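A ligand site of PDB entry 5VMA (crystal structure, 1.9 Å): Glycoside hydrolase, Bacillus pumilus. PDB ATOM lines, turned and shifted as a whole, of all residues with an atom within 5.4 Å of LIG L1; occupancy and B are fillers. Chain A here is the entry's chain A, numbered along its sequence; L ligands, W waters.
CB of Ala 39 touches C3 of LIG L1, 3.7 Å away. CD of Pro 40 touches O1 of LIG L1, at 3.8 Å. Thr 47 touches LIG L1 (CG2 to O1, 3.5 Å). CG of Trp 150 touches C11 of LIG L1, 3.3 Å away. Thr 223 touches LIG L1. Ala 225 touches LIG L1 (CB to O2, 3.5 Å). Tyr 296 touches LIG L1 (CB to O7, 3.5 Å). CG1 of Val 402 touches O13 of LIG L1, 3.6 Å away. 17 residues have an atom within 4 Å of LIG L1: Ala 39, Pro 40, Thr 47, Glu 49, Trp 150, Asn 174, Phe 176, Gln 177, Thr 223, Asn 224, Ala 225, Asp 227, Trp 295, Tyr 296, Tyr 322, Val 402 and Tyr 403.
The backbone NH (N) of Ser 48 is in hydrogen-bond range of the backbone carbonyl oxygen (O) of Trp 150 (2.9 Å). N of Glu 49 sits close to OG1 of Thr 47, at 3.3 Å. The backbone carbonyl oxygen (O) of Thr 223 sits at hydrogen-bond distance from the backbone NH (N) of Trp 150 (3.0 Å). The side-chain amide nitrogen (ND2) of Asn 174 sits at hydrogen-bond distance from the side-chain amide oxygen (OE1) of Gln 177, 3.3 Å away. OG1 of Thr 223 lies within hydrogen-bond range of OG of Ser 298, 2.7 Å away. OD1 of Asn 174 lies within hydrogen-bond range of NE1 of Trp 150 (3.0 Å).
An oxygen (O11) of LG2 L2 is in hydrogen-bond range of a nitrogen (N1) of LIG L1 (2.7 Å).
The backbone carbonyl oxygen (O) of Asn 224 is in hydrogen-bond range of an oxygen (O7) of LIG L1 (2.8 Å). The side-chain hydroxyl of Tyr 322 is in hydrogen-bond range of an oxygen (O3) of LIG L1 (3.3 Å). An oxygen (O10) of LG2 L2 lies within hydrogen-bond range of the side-chain carboxylate of Glu 49, at 2.7 Å. An oxygen (O10) of LIG L1 is in hydrogen-bond range of the backbone carbonyl oxygen (O) of Phe 176 (3.1 Å). NE1 of Trp 295 is in hydrogen-bond range of O5 of LIG L1, at 3.1 Å. The side-chain carboxylate (OD1) of Asp 227 is in hydrogen-bond range of an oxygen (O2) of LIG L1. The side-chain amide oxygen (OE1) of Gln 177 sits at hydrogen-bond distance from an oxygen (O10) of LIG L1 (2.8 Å). OH of Tyr 403 lies within hydrogen-bond range of O13 of LIG L1 (2.7 Å). OE1 of Glu 49 is in salt-bridge range of N1 of LIG L1 (3.2 Å). The side-chain amide oxygen of Asn 174 lies within hydrogen-bond range of an oxygen (O9) of LIG L1 (2.9 Å).
Water W9 lies within hydrogen-bond range of the side-chain hydroxyl (OG) of Ser 48, an oxygen (O2) of LIG L1 and the backbone NH (N) of Glu 49. Water W8 bridges N1 of LIG L1 (2.7 Å) and O11 of LG2 L2 (3.5 Å). Water W7 lies within hydrogen-bond range of the side-chain hydroxyl (OH) of Tyr 322 (2.6 Å), an oxygen (O6) of LIG L1 (2.8 Å) and the backbone carbonyl oxygen (O) of Trp 295 (2.9 Å). Water W1 bridges O11 of LIG L1 (2.8 Å) and OG of Ser 298 (2.9 Å). Water W2 lies within hydrogen-bond range of the side-chain hydroxyl (OH) of Tyr 322 (2.7 Å) and an oxygen (O4) of LIG L1 (3.1 Å). Water W5 lies within hydrogen-bond range of OD2 of Asp 227, OE1 of Glu 49 and O2 of LIG L1.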
ATOM      1  N   HIS A  30     -15.917  13.734 -15.391  1.00  0.00           N
ATOM      2  CA  HIS A  30     -16.778  12.660 -15.852  1.00  0.00           C
ATOM      3  C   HIS A  30     -16.322  11.308 -15.241  1.00  0.00           C
ATOM      4  O   HIS A  30     -17.153  10.500 -14.693  1.00  0.00           O
ATOM      5  CB  HIS A  30     -16.826  12.596 -17.352  1.00  0.00           C
ATOM      6  CG  HIS A  30     -17.613  11.432 -17.861  1.00  0.00           C
ATOM      7  ND1 HIS A  30     -19.000  11.387 -17.807  1.00  0.00           N
ATOM      8  CD2 HIS A  30     -17.200  10.268 -18.401  1.00  0.00           C
ATOM      9  CE1 HIS A  30     -19.389  10.220 -18.306  1.00  0.00           C
ATOM     10  NE2 HIS A  30     -18.325   9.527 -18.695  1.00  0.00           N
ATOM     11  N   ALA A  39     -20.517  10.301 -24.197  1.00  0.00           N
ATOM     12  CA  ALA A  39     -21.434  11.440 -24.371  1.00  0.00           C
ATOM     13  C   ALA A  39     -20.556  12.682 -24.255  1.00  0.00           C
ATOM     14  O   ALA A  39     -20.399  13.392 -25.273  1.00  0.00           O
ATOM     15  CB  ALA A  39     -22.626  11.358 -23.357  1.00  0.00           C
ATOM     16  N   PRO A  40     -19.824  12.867 -23.095  1.00  0.00           N
ATOM     17  CA  PRO A  40     -18.550  13.601 -23.229  1.00  0.00           C
ATOM     18  C   PRO A  40     -17.566  12.704 -24.015  1.00  0.00           C
ATOM     19  O   PRO A  40     -17.744  11.483 -24.076  1.00  0.00           O
ATOM     20  CB  PRO A  40     -18.118  13.852 -21.782  1.00  0.00           C
ATOM     21  CG  PRO A  40     -18.673  12.698 -21.045  1.00  0.00           C
ATOM     22  CD  PRO A  40     -19.978  12.322 -21.741  1.00  0.00           C
ATOM     23  N   THR A  47     -19.681  17.402 -16.754  1.00  0.00           N
ATOM     24  CA  THR A  47     -20.995  17.627 -17.286  1.00  0.00           C
ATOM     25  C   THR A  47     -21.904  18.227 -16.278  1.00  0.00           C
ATOM     26  O   THR A  47     -21.682  18.051 -15.062  1.00  0.00           O
ATOM     27  CB  THR A  47     -21.651  16.314 -17.751  1.00  0.00           C
ATOM     28  OG1 THR A  47     -21.746  15.430 -16.666  1.00  0.00           O
ATOM     29  CG2 THR A  47     -20.883  15.717 -18.827  1.00  0.00           C
ATOM     30  N   SER A  48     -22.993  18.833 -16.739  1.00  0.00           N
ATOM     31  CA  SER A  48     -24.042  19.234 -15.821  1.00  0.00           C
ATOM     32  C   SER A  48     -24.561  17.986 -15.064  1.00  0.00           C
ATOM     33  O   SER A  48     -24.937  18.086 -13.884  1.00  0.00           O
ATOM     34  CB  SER A  48     -25.162  20.084 -16.442  1.00  0.00           C
ATOM     35  OG  SER A  48     -25.679  19.520 -17.637  1.00  0.00           O
ATOM     36  N   GLU A  49     -24.603  16.835 -15.755  1.00  0.00           N
ATOM     37  CA  GLU A  49     -24.990  15.618 -15.151  1.00  0.00           C
ATOM     38  C   GLU A  49     -24.168  15.329 -13.898  1.00  0.00           C
ATOM     39  O   GLU A  49     -24.702  15.039 -12.796  1.00  0.00           O
ATOM     40  CB  GLU A  49     -24.853  14.502 -16.198  1.00  0.00           C
ATOM     41  CG  GLU A  49     -24.868  13.073 -15.678  1.00  0.00           C
ATOM     42  CD  GLU A  49     -24.632  12.167 -16.901  1.00  0.00           C
ATOM     43  OE1 GLU A  49     -25.604  11.858 -17.679  1.00  0.00           O
ATOM     44  OE2 GLU A  49     -23.408  11.855 -17.126  1.00  0.00           O
ATOM     45  N   TRP A 150     -23.927  22.428 -20.371  1.00  0.00           N
ATOM     46  CA  TRP A 150     -23.829  21.033 -20.113  1.00  0.00           C
ATOM     47  C   TRP A 150     -22.404  20.461 -20.051  1.00  0.00           C
ATOM     48  O   TRP A 150     -22.232  19.401 -19.493  1.00  0.00           O
ATOM     49  CB  TRP A 150     -24.644  20.248 -21.119  1.00  0.00           C
ATOM     50  CG  TRP A 150     -23.899  19.836 -22.444  1.00  0.00           C
ATOM     51  CD1 TRP A 150     -23.704  20.601 -23.503  1.00  0.00           C
ATOM     52  CD2 TRP A 150     -23.256  18.590 -22.722  1.00  0.00           C
ATOM     53  NE1 TRP A 150     -23.052  19.883 -24.514  1.00  0.00           N
ATOM     54  CE2 TRP A 150     -22.732  18.659 -24.038  1.00  0.00           C
ATOM     55  CE3 TRP A 150     -23.086  17.390 -22.003  1.00  0.00           C
ATOM     56  CZ2 TRP A 150     -22.025  17.564 -24.641  1.00  0.00           C
ATOM     57  CZ3 TRP A 150     -22.455  16.320 -22.621  1.00  0.00           C
ATOM     58  CH2 TRP A 150     -21.891  16.435 -23.906  1.00  0.00           C
ATOM     59  N   ASN A 174     -18.488  23.084 -26.435  1.00  0.00           N
ATOM     60  CA  ASN A 174     -19.591  22.295 -26.974  1.00  0.00           C
ATOM     61  C   ASN A 174     -19.099  21.390 -28.069  1.00  0.00           C
ATOM     62  O   ASN A 174     -17.999  21.605 -28.598  1.00  0.00           O
ATOM     63  CB  ASN A 174     -20.715  23.178 -27.475  1.00  0.00           C
ATOM     64  CG  ASN A 174     -22.110  22.461 -27.515  1.00  0.00           C
ATOM     65  OD1 ASN A 174     -22.296  21.296 -27.053  1.00  0.00           O
ATOM     66  ND2 ASN A 174     -23.106  23.188 -28.058  1.00  0.00           N
ATOM     67  N   PHE A 176     -21.732  18.528 -29.929  1.00  0.00           N
ATOM     68  CA  PHE A 176     -22.881  18.169 -30.826  1.00  0.00           C
ATOM     69  C   PHE A 176     -23.534  19.433 -31.366  1.00  0.00           C
ATOM     70  O   PHE A 176     -23.835  20.385 -30.583  1.00  0.00           O
ATOM     71  CB  PHE A 176     -23.969  17.454 -30.004  1.00  0.00           C
ATOM     72  CG  PHE A 176     -23.518  16.148 -29.408  1.00  0.00           C
ATOM     73  CD1 PHE A 176     -23.441  14.971 -30.209  1.00  0.00           C
ATOM     74  CD2 PHE A 176     -23.159  16.080 -28.064  1.00  0.00           C
ATOM     75  CE1 PHE A 176     -23.036  13.776 -29.656  1.00  0.00           C
ATOM     76  CE2 PHE A 176     -22.756  14.872 -27.546  1.00  0.00           C
ATOM     77  CZ  PHE A 176     -22.696  13.720 -28.321  1.00  0.00           C
ATOM     78  N   GLN A 177     -23.763  19.461 -32.677  1.00  0.00           N
ATOM     79  CA  GLN A 177     -24.479  20.561 -33.366  1.00  0.00           C
ATOM     80  C   GLN A 177     -25.228  20.137 -34.619  1.00  0.00           C
ATOM     81  O   GLN A 177     -26.054  20.898 -35.171  1.00  0.00           O
ATOM     82  CB  GLN A 177     -23.457  21.570 -33.912  1.00  0.00           C
ATOM     83  CG  GLN A 177     -22.749  22.423 -32.874  1.00  0.00           C
ATOM     84  CD  GLN A 177     -23.644  23.479 -32.298  1.00  0.00           C
ATOM     85  OE1 GLN A 177     -24.050  23.394 -31.178  1.00  0.00           O
ATOM     86  NE2 GLN A 177     -23.864  24.501 -33.037  1.00  0.00           N
ATOM     87  N   GLY A 179     -27.206  17.301 -35.710  1.00  0.00           N
ATOM     88  CA  GLY A 179     -28.363  16.490 -35.898  1.00  0.00           C
ATOM     89  C   GLY A 179     -28.216  15.075 -35.451  1.00  0.00           C
ATOM     90  O   GLY A 179     -27.254  14.682 -34.800  1.00  0.00           O
ATOM     91  N   THR A 223     -25.797  25.677 -23.988  1.00  0.00           N
ATOM     92  CA  THR A 223     -26.867  24.704 -24.058  1.00  0.00           C
ATOM     93  C   THR A 223     -26.933  23.922 -22.775  1.00  0.00           C
ATOM     94  O   THR A 223     -25.931  23.342 -22.349  1.00  0.00           O
ATOM     95  CB  THR A 223     -26.626  23.753 -25.264  1.00  0.00           C
ATOM     96  OG1 THR A 223     -26.518  24.518 -26.458  1.00  0.00           O
ATOM     97  CG2 THR A 223     -27.785  22.775 -25.390  1.00  0.00           C
ATOM     98  N   ASN A 224     -28.107  23.864 -22.122  1.00  0.00           N
ATOM     99  CA  ASN A 224     -28.293  23.019 -20.968  1.00  0.00           C
ATOM    100  C   ASN A 224     -28.670  21.610 -21.415  1.00  0.00           C
ATOM    101  O   ASN A 224     -29.010  21.393 -22.571  1.00  0.00           O
ATOM    102  CB  ASN A 224     -29.310  23.601 -19.954  1.00  0.00           C
ATOM    103  CG  ASN A 224     -30.731  23.140 -20.160  1.00  0.00           C
ATOM    104  OD1 ASN A 224     -31.193  23.072 -21.309  1.00  0.00           O
ATOM    105  ND2 ASN A 224     -31.444  22.811 -19.050  1.00  0.00           N
ATOM    106  N   ALA A 225     -28.690  20.714 -20.451  1.00  0.00           N
ATOM    107  CA  ALA A 225     -29.279  19.375 -20.541  1.00  0.00           C
ATOM    108  C   ALA A 225     -30.352  19.378 -19.449  1.00  0.00           C
ATOM    109  O   ALA A 225     -30.054  19.493 -18.272  1.00  0.00           O
ATOM    110  CB  ALA A 225     -28.207  18.364 -20.153  1.00  0.00           C
ATOM    111  N   ASP A 227     -32.326  17.282 -18.100  1.00  0.00           N
ATOM    112  CA  ASP A 227     -32.329  16.261 -17.053  1.00  0.00           C
ATOM    113  C   ASP A 227     -31.362  16.638 -15.930  1.00  0.00           C
ATOM    114  O   ASP A 227     -31.561  16.181 -14.796  1.00  0.00           O
ATOM    115  CB  ASP A 227     -32.019  14.808 -17.514  1.00  0.00           C
ATOM    116  CG  ASP A 227     -30.608  14.611 -18.105  1.00  0.00           C
ATOM    117  OD1 ASP A 227     -29.944  15.591 -18.544  1.00  0.00           O
ATOM    118  OD2 ASP A 227     -30.206  13.421 -18.169  1.00  0.00           O
ATOM    119  N   ALA A 228     -30.294  17.358 -16.250  1.00  0.00           N
ATOM    120  CA  ALA A 228     -29.287  17.697 -15.186  1.00  0.00           C
ATOM    121  C   ALA A 228     -29.732  18.764 -14.241  1.00  0.00           C
ATOM    122  O   ALA A 228     -29.638  18.600 -13.001  1.00  0.00           O
ATOM    123  CB  ALA A 228     -27.927  18.051 -15.777  1.00  0.00           C
ATOM    124  N   TRP A 295     -35.096  18.091 -24.956  1.00  0.00           N
ATOM    125  CA  TRP A 295     -33.725  17.668 -24.811  1.00  0.00           C
ATOM    126  C   TRP A 295     -32.791  18.787 -24.268  1.00  0.00           C
ATOM    127  O   TRP A 295     -31.784  18.521 -23.568  1.00  0.00           O
ATOM    128  CB  TRP A 295     -33.240  17.239 -26.221  1.00  0.00           C
ATOM    129  CG  TRP A 295     -31.983  16.480 -26.280  1.00  0.00           C
ATOM    130  CD1 TRP A 295     -30.760  16.910 -26.820  1.00  0.00           C
ATOM    131  CD2 TRP A 295     -31.826  15.075 -26.095  1.00  0.00           C
ATOM    132  NE1 TRP A 295     -29.887  15.924 -26.790  1.00  0.00           N
ATOM    133  CE2 TRP A 295     -30.509  14.756 -26.405  1.00  0.00           C
ATOM    134  CE3 TRP A 295     -32.684  14.061 -25.664  1.00  0.00           C
ATOM    135  CZ2 TRP A 295     -29.996  13.456 -26.323  1.00  0.00           C
ATOM    136  CZ3 TRP A 295     -32.157  12.734 -25.515  1.00  0.00           C
ATOM    137  CH2 TRP A 295     -30.845  12.448 -25.891  1.00  0.00           C
ATOM    138  N   TYR A 296     -33.081  20.030 -24.650  1.00  0.00           N
ATOM    139  CA  TYR A 296     -32.313  21.175 -24.227  1.00  0.00           C
ATOM    140  C   TYR A 296     -33.059  22.510 -24.408  1.00  0.00           C
ATOM    141  O   TYR A 296     -34.088  22.530 -25.045  1.00  0.00           O
ATOM    142  CB  TYR A 296     -30.983  21.234 -25.080  1.00  0.00           C
ATOM    143  CG  TYR A 296     -31.288  21.429 -26.538  1.00  0.00           C
ATOM    144  CD1 TYR A 296     -31.496  20.339 -27.322  1.00  0.00           C
ATOM    145  CD2 TYR A 296     -31.340  22.691 -27.114  1.00  0.00           C
ATOM    146  CE1 TYR A 296     -31.736  20.442 -28.664  1.00  0.00           C
ATOM    147  CE2 TYR A 296     -31.612  22.864 -28.483  1.00  0.00           C
ATOM    148  CZ  TYR A 296     -31.833  21.683 -29.251  1.00  0.00           C
ATOM    149  OH  TYR A 296     -32.143  21.779 -30.528  1.00  0.00           O
ATOM    150  N   SER A 298     -31.164  26.353 -25.584  1.00  0.00           N
ATOM    151  CA  SER A 298     -29.939  27.049 -25.884  1.00  0.00           C
ATOM    152  C   SER A 298     -30.184  28.555 -25.902  1.00  0.00           C
ATOM    153  O   SER A 298     -31.296  29.012 -26.133  1.00  0.00           O
ATOM    154  CB  SER A 298     -29.298  26.651 -27.232  1.00  0.00           C
ATOM    155  OG  SER A 298     -28.940  25.272 -27.287  1.00  0.00           O
ATOM    156  N   TYR A 322     -35.556  11.833 -19.848  1.00  0.00           N
ATOM    157  CA  TYR A 322     -35.222  13.137 -19.316  1.00  0.00           C
ATOM    158  C   TYR A 322     -36.264  13.706 -18.353  1.00  0.00           C
ATOM    159  O   TYR A 322     -35.971  14.697 -17.694  1.00  0.00           O
ATOM    160  CB  TYR A 322     -35.047  14.126 -20.476  1.00  0.00           C
ATOM    161  CG  TYR A 322     -33.704  14.144 -21.114  1.00  0.00           C
ATOM    162  CD1 TYR A 322     -33.057  12.975 -21.507  1.00  0.00           C
ATOM    163  CD2 TYR A 322     -33.099  15.349 -21.423  1.00  0.00           C
ATOM    164  CE1 TYR A 322     -31.767  13.019 -22.129  1.00  0.00           C
ATOM    165  CE2 TYR A 322     -31.857  15.407 -21.999  1.00  0.00           C
ATOM    166  CZ  TYR A 322     -31.171  14.245 -22.326  1.00  0.00           C
ATOM    167  OH  TYR A 322     -29.970  14.315 -22.955  1.00  0.00           O
ATOM    168  N   VAL A 402     -34.123  12.448 -30.987  1.00  0.00           N
ATOM    169  CA  VAL A 402     -32.931  13.272 -31.123  1.00  0.00           C
ATOM    170  C   VAL A 402     -31.771  12.546 -31.738  1.00  0.00           C
ATOM    171  O   VAL A 402     -31.160  13.135 -32.595  1.00  0.00           O
ATOM    172  CB  VAL A 402     -32.422  13.967 -29.827  1.00  0.00           C
ATOM    173  CG1 VAL A 402     -31.505  15.136 -30.167  1.00  0.00           C
ATOM    174  CG2 VAL A 402     -33.558  14.547 -29.014  1.00  0.00           C
ATOM    175  N   TYR A 403     -31.396  11.332 -31.279  1.00  0.00           N
ATOM    176  CA  TYR A 403     -30.198  10.652 -31.836  1.00  0.00           C
ATOM    177  C   TYR A 403     -30.536   9.276 -32.316  1.00  0.00           C
ATOM    178  O   TYR A 403     -31.252   8.571 -31.620  1.00  0.00           O
ATOM    179  CB  TYR A 403     -29.038  10.545 -30.831  1.00  0.00           C
ATOM    180  CG  TYR A 403     -28.423  11.896 -30.703  1.00  0.00           C
ATOM    181  CD1 TYR A 403     -27.453  12.364 -31.648  1.00  0.00           C
ATOM    182  CD2 TYR A 403     -28.768  12.747 -29.672  1.00  0.00           C
ATOM    183  CE1 TYR A 403     -26.918  13.658 -31.568  1.00  0.00           C
ATOM    184  CE2 TYR A 403     -28.245  14.060 -29.587  1.00  0.00           C
ATOM    185  CZ  TYR A 403     -27.332  14.506 -30.549  1.00  0.00           C
ATOM    186  OH  TYR A 403     -26.828  15.796 -30.486  1.00  0.00           O
ATOM    187  N   TRP A 417     -32.980   5.259 -14.961  1.00  0.00           N
ATOM    188  CA  TRP A 417     -32.937   6.625 -14.454  1.00  0.00           C
ATOM    189  C   TRP A 417     -34.361   7.280 -14.242  1.00  0.00           C
ATOM    190  O   TRP A 417     -34.585   7.890 -13.193  1.00  0.00           O
ATOM    191  CB  TRP A 417     -32.064   7.531 -15.371  1.00  0.00           C
ATOM    192  CG  TRP A 417     -30.567   7.405 -15.190  1.00  0.00           C
ATOM    193  CD1 TRP A 417     -29.906   6.762 -14.172  1.00  0.00           C
ATOM    194  CD2 TRP A 417     -29.584   8.039 -15.961  1.00  0.00           C
ATOM    195  NE1 TRP A 417     -28.535   6.914 -14.322  1.00  0.00           N
ATOM    196  CE2 TRP A 417     -28.312   7.695 -15.422  1.00  0.00           C
ATOM    197  CE3 TRP A 417     -29.643   8.906 -17.072  1.00  0.00           C
ATOM    198  CZ2 TRP A 417     -27.109   8.225 -15.917  1.00  0.00           C
ATOM    199  CZ3 TRP A 417     -28.450   9.382 -17.630  1.00  0.00           C
ATOM    200  CH2 TRP A 417     -27.190   9.052 -17.036  1.00  0.00           C
HETATM  201  O1  LIG L   1     -23.188  13.392 -20.067  1.00  0.00           O
HETATM  202  C1  LIG L   1     -24.335  14.245 -20.052  1.00  0.00           C
HETATM  203  C2  LIG L   1     -25.105  14.040 -21.356  1.00  0.00           C
HETATM  204  C3  LIG L   1     -25.664  12.610 -21.554  1.00  0.00           C
HETATM  205  N1  LIG L   1     -26.824  12.379 -20.640  1.00  0.00           N
HETATM  206  C4  LIG L   1     -27.921  13.343 -20.496  1.00  0.00           C
HETATM  207  C5  LIG L   1     -27.450  14.773 -20.432  1.00  0.00           C
HETATM  208  O2  LIG L   1     -27.092  15.215 -19.048  1.00  0.00           O
HETATM  209  C6  LIG L   1     -26.226  15.079 -21.437  1.00  0.00           C
HETATM  210  O3  LIG L   1     -26.733  15.007 -22.795  1.00  0.00           O
HETATM  211  C7  LIG L   1     -26.265  15.841 -23.749  1.00  0.00           C
HETATM  212  C8  LIG L   1     -26.753  15.266 -25.098  1.00  0.00           C
HETATM  213  O4  LIG L   1     -26.230  13.949 -25.191  1.00  0.00           O
HETATM  214  C9  LIG L   1     -26.197  16.126 -26.216  1.00  0.00           C
HETATM  215  O5  LIG L   1     -26.849  15.733 -27.448  1.00  0.00           O
HETATM  216  O6  LIG L   1     -26.746  17.159 -23.567  1.00  0.00           O
HETATM  217  C10 LIG L   1     -26.141  17.969 -24.559  1.00  0.00           C
HETATM  218  C11 LIG L   1     -26.725  19.332 -24.138  1.00  0.00           C
HETATM  219  O7  LIG L   1     -28.163  19.330 -24.297  1.00  0.00           O
HETATM  220  C12 LIG L   1     -26.596  17.548 -25.938  1.00  0.00           C
HETATM  221  O8  LIG L   1     -25.920  18.364 -26.797  1.00  0.00           O
HETATM  222  C13 LIG L   1     -26.694  19.298 -27.506  1.00  0.00           C
HETATM  223  C14 LIG L   1     -25.815  20.435 -28.039  1.00  0.00           C
HETATM  224  O9  LIG L   1     -25.200  21.157 -27.033  1.00  0.00           O
HETATM  225  C15 LIG L   1     -26.729  21.405 -28.832  1.00  0.00           C
HETATM  226  O10 LIG L   1     -25.911  22.364 -29.407  1.00  0.00           O
HETATM  227  C16 LIG L   1     -27.365  20.665 -29.896  1.00  0.00           C
HETATM  228  O11 LIG L   1     -28.300  21.552 -30.610  1.00  0.00           O
HETATM  229  O12 LIG L   1     -27.315  18.608 -28.577  1.00  0.00           O
HETATM  230  C17 LIG L   1     -28.202  19.463 -29.350  1.00  0.00           C
HETATM  231  C18 LIG L   1     -28.849  18.955 -30.578  1.00  0.00           C
HETATM  232  O13 LIG L   1     -28.842  17.574 -30.562  1.00  0.00           O
HETATM  233  O1  LG2 L   2     -20.325  -0.485 -24.776  1.00  0.00           O
HETATM  234  C1  LG2 L   2     -21.590  -0.837 -24.384  1.00  0.00           C
HETATM  235  C2  LG2 L   2     -21.584  -1.428 -23.002  1.00  0.00           C
HETATM  236  C3  LG2 L   2     -20.443  -2.598 -22.831  1.00  0.00           C
HETATM  237  N1  LG2 L   2     -20.990  -3.330 -21.659  1.00  0.00           N
HETATM  238  C4  LG2 L   2     -21.100  -2.528 -20.423  1.00  0.00           C
HETATM  239  C5  LG2 L   2     -21.930  -1.229 -20.581  1.00  0.00           C
HETATM  240  O2  LG2 L   2     -21.830  -0.488 -19.376  1.00  0.00           O
HETATM  241  C6  LG2 L   2     -21.575  -0.400 -21.821  1.00  0.00           C
HETATM  242  O3  LG2 L   2     -22.690   0.567 -21.998  1.00  0.00           O
HETATM  243  C7  LG2 L   2     -22.314   1.863 -21.888  1.00  0.00           C
HETATM  244  C8  LG2 L   2     -23.372   2.641 -22.551  1.00  0.00           C
HETATM  245  O4  LG2 L   2     -23.449   2.390 -23.926  1.00  0.00           O
HETATM  246  C9  LG2 L   2     -23.033   4.135 -22.394  1.00  0.00           C
HETATM  247  O5  LG2 L   2     -24.097   4.858 -22.950  1.00  0.00           O
HETATM  248  O6  LG2 L   2     -22.316   2.197 -20.508  1.00  0.00           O
HETATM  249  C10 LG2 L   2     -21.890   3.517 -20.281  1.00  0.00           C
HETATM  250  C11 LG2 L   2     -21.785   3.695 -18.788  1.00  0.00           C
HETATM  251  O7  LG2 L   2     -23.019   3.542 -18.087  1.00  0.00           O
HETATM  252  C12 LG2 L   2     -22.888   4.490 -20.903  1.00  0.00           C
HETATM  253  O8  LG2 L   2     -22.348   5.805 -20.717  1.00  0.00           O
HETATM  254  C13 LG2 L   2     -23.345   6.760 -20.345  1.00  0.00           C
HETATM  255  C14 LG2 L   2     -22.572   8.035 -19.826  1.00  0.00           C
HETATM  256  O9  LG2 L   2     -21.577   7.620 -18.889  1.00  0.00           O
HETATM  257  C15 LG2 L   2     -23.461   9.049 -19.298  1.00  0.00           C
HETATM  258  O10 LG2 L   2     -22.746  10.264 -19.145  1.00  0.00           O
HETATM  259  C16 LG2 L   2     -24.582   9.281 -20.319  1.00  0.00           C
HETATM  260  O11 LG2 L   2     -25.603  10.110 -19.753  1.00  0.00           O
HETATM  261  O12 LG2 L   2     -24.207   7.123 -21.327  1.00  0.00           O
HETATM  262  C17 LG2 L   2     -25.244   7.941 -20.776  1.00  0.00           C
HETATM  263  C18 LG2 L   2     -26.344   8.244 -21.726  1.00  0.00           C
HETATM  264  O13 LG2 L   2     -25.781   8.855 -22.850  1.00  0.00           O
HETATM  265  O   HOH W   1     -28.269  24.208 -29.854  1.00  0.00           O
HETATM  266  O   HOH W   2     -28.331  12.250 -23.688  1.00  0.00           O
HETATM  267  O   HOH W   3     -26.051  12.302 -27.545  1.00  0.00           O
HETATM  268  O   HOH W   4     -30.947  17.752 -32.561  1.00  0.00           O
HETATM  269  O   HOH W   5     -27.900  13.041 -16.716  1.00  0.00           O
HETATM  270  O   HOH W   6     -29.728  23.670 -32.396  1.00  0.00           O
HETATM  271  O   HOH W   7     -29.480  16.843 -23.450  1.00  0.00           O
HETATM  272  O   HOH W   8     -28.679  10.465 -21.289  1.00  0.00           O
HETATM  273  O   HOH W   9     -25.138  17.099 -18.730  1.00  0.00           O
